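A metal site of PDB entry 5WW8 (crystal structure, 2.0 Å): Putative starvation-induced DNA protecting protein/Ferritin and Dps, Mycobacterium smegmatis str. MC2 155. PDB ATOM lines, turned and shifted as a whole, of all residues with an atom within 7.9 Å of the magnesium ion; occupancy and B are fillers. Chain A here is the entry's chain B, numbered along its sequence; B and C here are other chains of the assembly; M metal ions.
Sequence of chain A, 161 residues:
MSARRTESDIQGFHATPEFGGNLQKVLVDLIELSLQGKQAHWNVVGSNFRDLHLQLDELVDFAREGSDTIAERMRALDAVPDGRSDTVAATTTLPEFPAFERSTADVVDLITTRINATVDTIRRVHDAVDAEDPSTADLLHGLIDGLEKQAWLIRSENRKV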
ATOM      1  N   SER A  47       3.058   7.648 -17.194  1.00  0.00           N
ATOM      2  CA  SER A  47       4.413   8.197 -17.076  1.00  0.00           C
ATOM      3  C   SER A  47       4.457   9.438 -16.226  1.00  0.00           C
ATOM      4  O   SER A  47       3.673  10.364 -16.452  1.00  0.00           O
ATOM      5  CB  SER A  47       4.945   8.550 -18.472  1.00  0.00           C
ATOM      6  OG  SER A  47       4.636   7.494 -19.366  1.00  0.00           O
ATOM      7  N   ASN A  48       5.381   9.464 -15.274  1.00  0.00           N
ATOM      8  CA  ASN A  48       5.528  10.555 -14.301  1.00  0.00           C
ATOM      9  C   ASN A  48       4.297  10.777 -13.405  1.00  0.00           C
ATOM     10  O   ASN A  48       3.971  11.909 -13.015  1.00  0.00           O
ATOM     11  CB  ASN A  48       5.971  11.866 -14.982  1.00  0.00           C
ATOM     12  CG  ASN A  48       6.658  12.794 -14.014  1.00  0.00           C
ATOM     13  OD1 ASN A  48       7.231  12.348 -13.025  1.00  0.00           O
ATOM     14  ND2 ASN A  48       6.607  14.096 -14.287  1.00  0.00           N
ATOM     15  N   PHE A  49       3.633   9.659 -13.087  1.00  0.00           N
ATOM     16  CA  PHE A  49       2.491   9.642 -12.176  1.00  0.00           C
ATOM     17  C   PHE A  49       2.756  10.413 -10.883  1.00  0.00           C
ATOM     18  O   PHE A  49       1.982  11.267 -10.492  1.00  0.00           O
ATOM     19  CB  PHE A  49       2.103   8.184 -11.844  1.00  0.00           C
ATOM     20  CG  PHE A  49       1.238   8.075 -10.622  1.00  0.00           C
ATOM     21  CD1 PHE A  49      -0.136   8.360 -10.693  1.00  0.00           C
ATOM     22  CD2 PHE A  49       1.788   7.702  -9.392  1.00  0.00           C
ATOM     23  CE1 PHE A  49      -0.931   8.276  -9.549  1.00  0.00           C
ATOM     24  CE2 PHE A  49       0.998   7.607  -8.254  1.00  0.00           C
ATOM     25  CZ  PHE A  49      -0.365   7.902  -8.334  1.00  0.00           C
ATOM     26  N   ARG A  50       3.869  10.088 -10.223  1.00  0.00           N
ATOM     27  CA  ARG A  50       4.090  10.548  -8.859  1.00  0.00           C
ATOM     28  C   ARG A  50       4.204  12.089  -8.754  1.00  0.00           C
ATOM     29  O   ARG A  50       3.553  12.676  -7.895  1.00  0.00           O
ATOM     30  CB  ARG A  50       5.295   9.829  -8.237  1.00  0.00           C
ATOM     31  CG  ARG A  50       5.522  10.166  -6.777  1.00  0.00           C
ATOM     32  CD  ARG A  50       6.732   9.447  -6.245  1.00  0.00           C
ATOM     33  NE  ARG A  50       7.019   9.867  -4.878  1.00  0.00           N
ATOM     34  CZ  ARG A  50       7.750  10.938  -4.557  1.00  0.00           C
ATOM     35  NH1 ARG A  50       8.282  11.708  -5.503  1.00  0.00           N
ATOM     36  NH2 ARG A  50       7.931  11.243  -3.283  1.00  0.00           N
ATOM     37  N   ASP A  51       4.994  12.701  -9.631  1.00  0.00           N
ATOM     38  CA  ASP A  51       5.153  14.165  -9.694  1.00  0.00           C
ATOM     39  C   ASP A  51       3.813  14.869  -9.861  1.00  0.00           C
ATOM     40  O   ASP A  51       3.572  15.890  -9.203  1.00  0.00           O
ATOM     41  CB  ASP A  51       6.050  14.567 -10.871  1.00  0.00           C
ATOM     42  CG  ASP A  51       7.528  14.693 -10.495  1.00  0.00           C
ATOM     43  OD1 ASP A  51       7.860  15.110  -9.363  1.00  0.00           O
ATOM     44  OD2 ASP A  51       8.376  14.383 -11.355  1.00  0.00           O
ATOM     45  N   LEU A  52       2.974  14.340 -10.745  1.00  0.00           N
ATOM     46  CA  LEU A  52       1.643  14.915 -10.977  1.00  0.00           C
ATOM     47  C   LEU A  52       0.712  14.703  -9.803  1.00  0.00           C
ATOM     48  O   LEU A  52       0.053  15.656  -9.374  1.00  0.00           O
ATOM     49  CB  LEU A  52       1.009  14.378 -12.272  1.00  0.00           C
ATOM     50  CG  LEU A  52       1.095  15.232 -13.538  1.00  0.00           C
ATOM     51  CD1 LEU A  52       0.364  16.564 -13.340  1.00  0.00           C
ATOM     52  CD2 LEU A  52       2.537  15.449 -14.023  1.00  0.00           C
ATOM     53  N   GLU A 157       5.323  20.054 -17.954  1.00  0.00           N
ATOM     54  CA  GLU A 157       5.421  18.614 -18.239  1.00  0.00           C
ATOM     55  C   GLU A 157       5.155  18.231 -19.715  1.00  0.00           C
ATOM     56  O   GLU A 157       5.755  17.277 -20.224  1.00  0.00           O
ATOM     57  CB  GLU A 157       4.475  17.844 -17.298  1.00  0.00           C
ATOM     58  CG  GLU A 157       4.370  16.329 -17.505  1.00  0.00           C
ATOM     59  CD  GLU A 157       5.614  15.551 -17.087  1.00  0.00           C
ATOM     60  OE1 GLU A 157       5.752  14.393 -17.535  1.00  0.00           O
ATOM     61  OE2 GLU A 157       6.442  16.083 -16.312  1.00  0.00           O
ATOM     62  N   SER B  47       9.172  16.398 -20.336  1.00  0.00           N
ATOM     63  CA  SER B  47       8.894  15.173 -19.552  1.00  0.00           C
ATOM     64  C   SER B  47       9.677  15.129 -18.260  1.00  0.00           C
ATOM     65  O   SER B  47      10.888  15.315 -18.270  1.00  0.00           O
ATOM     66  CB  SER B  47       9.220  13.923 -20.359  1.00  0.00           C
ATOM     67  OG  SER B  47       8.418  13.858 -21.509  1.00  0.00           O
ATOM     68  N   ASN B  48       8.977  14.831 -17.169  1.00  0.00           N
ATOM     69  CA  ASN B  48       9.550  14.795 -15.825  1.00  0.00           C
ATOM     70  C   ASN B  48      10.113  16.140 -15.353  1.00  0.00           C
ATOM     71  O   ASN B  48      11.100  16.188 -14.603  1.00  0.00           O
ATOM     72  CB  ASN B  48      10.589  13.650 -15.660  1.00  0.00           C
ATOM     73  CG  ASN B  48      10.701  13.186 -14.218  1.00  0.00           C
ATOM     74  OD1 ASN B  48       9.764  13.345 -13.437  1.00  0.00           O
ATOM     75  ND2 ASN B  48      11.855  12.640 -13.852  1.00  0.00           N
ATOM     76  N   PHE B  49       9.475  17.230 -15.817  1.00  0.00           N
ATOM     77  CA  PHE B  49       9.776  18.602 -15.376  1.00  0.00           C
ATOM     78  C   PHE B  49       9.966  18.712 -13.861  1.00  0.00           C
ATOM     79  O   PHE B  49      10.998  19.215 -13.417  1.00  0.00           O
ATOM     80  CB  PHE B  49       8.674  19.597 -15.815  1.00  0.00           C
ATOM     81  CG  PHE B  49       8.736  20.930 -15.093  1.00  0.00           C
ATOM     82  CD1 PHE B  49       7.845  21.229 -14.051  1.00  0.00           C
ATOM     83  CD2 PHE B  49       9.715  21.881 -15.435  1.00  0.00           C
ATOM     84  CE1 PHE B  49       7.914  22.453 -13.382  1.00  0.00           C
ATOM     85  CE2 PHE B  49       9.784  23.105 -14.766  1.00  0.00           C
ATOM     86  CZ  PHE B  49       8.884  23.391 -13.740  1.00  0.00           C
ATOM     87  N   ARG B  50       8.975  18.273 -13.090  1.00  0.00           N
ATOM     88  CA  ARG B  50       8.943  18.564 -11.651  1.00  0.00           C
ATOM     89  C   ARG B  50      10.141  17.979 -10.896  1.00  0.00           C
ATOM     90  O   ARG B  50      10.799  18.692 -10.138  1.00  0.00           O
ATOM     91  CB  ARG B  50       7.610  18.117 -11.026  1.00  0.00           C
ATOM     92  CG  ARG B  50       7.441  18.515  -9.568  1.00  0.00           C
ATOM     93  CD  ARG B  50       6.086  18.061  -9.044  1.00  0.00           C
ATOM     94  NE  ARG B  50       5.957  18.325  -7.613  1.00  0.00           N
ATOM     95  CZ  ARG B  50       6.404  17.535  -6.645  1.00  0.00           C
ATOM     96  NH1 ARG B  50       7.035  16.390  -6.915  1.00  0.00           N
ATOM     97  NH2 ARG B  50       6.220  17.886  -5.398  1.00  0.00           N
ATOM     98  N   ASP B  51      10.415  16.690 -11.105  1.00  0.00           N
ATOM     99  CA  ASP B  51      11.567  16.006 -10.513  1.00  0.00           C
ATOM    100  C   ASP B  51      12.853  16.759 -10.767  1.00  0.00           C
ATOM    101  O   ASP B  51      13.639  16.981  -9.843  1.00  0.00           O
ATOM    102  CB  ASP B  51      11.712  14.593 -11.051  1.00  0.00           C
ATOM    103  CG  ASP B  51      11.054  13.567 -10.172  1.00  0.00           C
ATOM    104  OD1 ASP B  51      11.058  13.735  -8.923  1.00  0.00           O
ATOM    105  OD2 ASP B  51      10.531  12.580 -10.737  1.00  0.00           O
ATOM    106  N   LEU B  52      13.049  17.163 -12.034  1.00  0.00           N
ATOM    107  CA  LEU B  52      14.233  17.932 -12.421  1.00  0.00           C
ATOM    108  C   LEU B  52      14.268  19.319 -11.803  1.00  0.00           C
ATOM    109  O   LEU B  52      15.286  19.719 -11.237  1.00  0.00           O
ATOM    110  CB  LEU B  52      14.362  18.012 -13.957  1.00  0.00           C
ATOM    111  CG  LEU B  52      15.384  17.096 -14.645  1.00  0.00           C
ATOM    112  CD1 LEU B  52      16.788  17.327 -14.083  1.00  0.00           C
ATOM    113  CD2 LEU B  52      14.960  15.628 -14.560  1.00  0.00           C
ATOM    114  N   GLU B 157      18.292   9.930 -14.859  1.00  0.00           N
ATOM    115  CA  GLU B 157      17.149  10.260 -15.725  1.00  0.00           C
ATOM    116  C   GLU B 157      17.346   9.855 -17.191  1.00  0.00           C
ATOM    117  O   GLU B 157      16.433   9.303 -17.804  1.00  0.00           O
ATOM    118  CB  GLU B 157      16.816  11.755 -15.619  1.00  0.00           C
ATOM    119  CG  GLU B 157      15.692  12.263 -16.515  1.00  0.00           C
ATOM    120  CD  GLU B 157      14.314  11.651 -16.232  1.00  0.00           C
ATOM    121  OE1 GLU B 157      14.002  11.321 -15.055  1.00  0.00           O
ATOM    122  OE2 GLU B 157      13.535  11.503 -17.201  1.00  0.00           O
ATOM    123  N   SER C  47      14.074   6.927 -17.279  1.00  0.00           N
ATOM    124  CA  SER C  47      12.997   7.901 -17.272  1.00  0.00           C
ATOM    125  C   SER C  47      12.229   7.905 -15.944  1.00  0.00           C
ATOM    126  O   SER C  47      11.807   6.853 -15.467  1.00  0.00           O
ATOM    127  CB  SER C  47      12.068   7.612 -18.452  1.00  0.00           C
ATOM    128  OG  SER C  47      11.155   8.673 -18.623  1.00  0.00           O
ATOM    129  N   ASN C  48      12.086   9.093 -15.368  1.00  0.00           N
ATOM    130  CA  ASN C  48      11.447   9.290 -14.048  1.00  0.00           C
ATOM    131  C   ASN C  48      12.171   8.603 -12.877  1.00  0.00           C
ATOM    132  O   ASN C  48      11.541   8.138 -11.900  1.00  0.00           O
ATOM    133  CB  ASN C  48       9.939   8.958 -14.090  1.00  0.00           C
ATOM    134  CG  ASN C  48       9.179   9.633 -12.968  1.00  0.00           C
ATOM    135  OD1 ASN C  48       9.566  10.721 -12.511  1.00  0.00           O
ATOM    136  ND2 ASN C  48       8.106   9.001 -12.490  1.00  0.00           N
ATOM    137  N   PHE C  49      13.500   8.566 -12.970  1.00  0.00           N
ATOM    138  CA  PHE C  49      14.372   8.043 -11.925  1.00  0.00           C
ATOM    139  C   PHE C  49      14.019   8.589 -10.531  1.00  0.00           C
ATOM    140  O   PHE C  49      13.887   7.817  -9.588  1.00  0.00           O
ATOM    141  CB  PHE C  49      15.846   8.351 -12.214  1.00  0.00           C
ATOM    142  CG  PHE C  49      16.733   8.228 -11.001  1.00  0.00           C
ATOM    143  CD1 PHE C  49      17.141   6.963 -10.559  1.00  0.00           C
ATOM    144  CD2 PHE C  49      17.126   9.358 -10.288  1.00  0.00           C
ATOM    145  CE1 PHE C  49      17.948   6.835  -9.424  1.00  0.00           C
ATOM    146  CE2 PHE C  49      17.927   9.241  -9.147  1.00  0.00           C
ATOM    147  CZ  PHE C  49      18.343   7.979  -8.716  1.00  0.00           C
ATOM    148  N   ARG C  50      13.902   9.922 -10.418  1.00  0.00           N
ATOM    149  CA  ARG C  50      13.827  10.568  -9.127  1.00  0.00           C
ATOM    150  C   ARG C  50      12.574  10.152  -8.344  1.00  0.00           C
ATOM    151  O   ARG C  50      12.691   9.741  -7.180  1.00  0.00           O
ATOM    152  CB  ARG C  50      13.948  12.088  -9.257  1.00  0.00           C
ATOM    153  CG  ARG C  50      14.114  12.801  -7.919  1.00  0.00           C
ATOM    154  CD  ARG C  50      14.177  14.314  -8.088  1.00  0.00           C
ATOM    155  NE  ARG C  50      14.175  14.970  -6.781  1.00  0.00           N
ATOM    156  CZ  ARG C  50      13.083  15.373  -6.126  1.00  0.00           C
ATOM    157  NH1 ARG C  50      11.865  15.209  -6.644  1.00  0.00           N
ATOM    158  NH2 ARG C  50      13.213  15.947  -4.950  1.00  0.00           N
ATOM    159  N   ASP C  51      11.408  10.224  -8.982  1.00  0.00           N
ATOM    160  CA  ASP C  51      10.146   9.792  -8.351  1.00  0.00           C
ATOM    161  C   ASP C  51      10.236   8.366  -7.841  1.00  0.00           C
ATOM    162  O   ASP C  51       9.856   8.096  -6.691  1.00  0.00           O
ATOM    163  CB  ASP C  51       8.958   9.880  -9.314  1.00  0.00           C
ATOM    164  CG  ASP C  51       8.282  11.233  -9.307  1.00  0.00           C
ATOM    165  OD1 ASP C  51       8.115  11.867  -8.230  1.00  0.00           O
ATOM    166  OD2 ASP C  51       7.884  11.652 -10.407  1.00  0.00           O
ATOM    167  N   LEU C  52      10.746   7.459  -8.683  1.00  0.00           N
ATOM    168  CA  LEU C  52      10.882   6.050  -8.319  1.00  0.00           C
ATOM    169  C   LEU C  52      11.866   5.829  -7.193  1.00  0.00           C
ATOM    170  O   LEU C  52      11.571   5.118  -6.236  1.00  0.00           O
ATOM    171  CB  LEU C  52      11.229   5.181  -9.541  1.00  0.00           C
ATOM    172  CG  LEU C  52      10.068   4.468 -10.244  1.00  0.00           C
ATOM    173  CD1 LEU C  52       9.342   3.527  -9.278  1.00  0.00           C
ATOM    174  CD2 LEU C  52       9.086   5.461 -10.886  1.00  0.00           C
ATOM    175  N   GLU C 157       2.748   4.367 -12.553  1.00  0.00           N
ATOM    176  CA  GLU C 157       3.780   4.823 -13.491  1.00  0.00           C
ATOM    177  C   GLU C 157       3.729   4.098 -14.832  1.00  0.00           C
ATOM    178  O   GLU C 157       3.895   4.728 -15.884  1.00  0.00           O
ATOM    179  CB  GLU C 157       5.161   4.691 -12.841  1.00  0.00           C
ATOM    180  CG  GLU C 157       6.367   4.942 -13.763  1.00  0.00           C
ATOM    181  CD  GLU C 157       6.510   6.385 -14.238  1.00  0.00           C
ATOM    182  OE1 GLU C 157       7.166   6.587 -15.278  1.00  0.00           O
ATOM    183  OE2 GLU C 157       5.996   7.320 -13.573  1.00  0.00           O
HETATM  184 MG    MG M   1       8.923  12.519 -11.902  1.00  0.00          MG
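OD1 of Asp 51 of chain C is in salt-bridge range of NH1 of Arg 50 of chain A. OE2 of Glu 157 of chain C sits at hydrogen-bond distance from N of Asn 48 of chain A (2.8 Å). ND2 of Asn 48 of chain B is in hydrogen-bond range of OE1 of Glu 157 of chain B. The side-chain carboxylate (OD1) of Asp 51 of chain B lies within salt-bridge range of the guanidinium group (NH1) of Arg 50 of chain C. The side-chain carboxylate (OE2) of Glu 157 of chain A sits at hydrogen-bond distance from the backbone NH (N) of Asn 48 of chain B, 3.0 Å away. NH1 of Arg 50 of chain B lies within salt-bridge range of OD1 of Asp 51 of chain A. The side-chain carboxylate of Glu 157 of chain A sits at hydrogen-bond distance from the side-chain amide nitrogen of Asn 48 of chain A (2.8 Å). ND2 of Asn 48 of chain C lies within hydrogen-bond range of OE2 of Glu 157 of chain C (2.9 Å).
Six residues have an atom within 4 Å of the magnesium ion: Asn 48 of chain A, Asp 51 of chain A, Asn 48 of chain B, Asp 51 of chain B, Asn 48 of chain C and Asp 51 of chain C. Along chain A the residues within 4 Å of the magnesium ion span positions 48 to 51. The nearest printed residue that does not touch the magnesium ion is Arg 50 of chain C (5.6 Å).
The magnesium ion is bound by OD1 of Asn 48 of chain B (1.9 Å), OD2 of Asp 51 of chain B (2.0 Å), OD1 of Asn 48 of chain C (2.0 Å), OD2 of Asp 51 of chain C (2.0 Å), OD2 of Asp 51 of chain A (2.0 Å) and OD1 of Asn 48 of chain A (2.0 Å).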
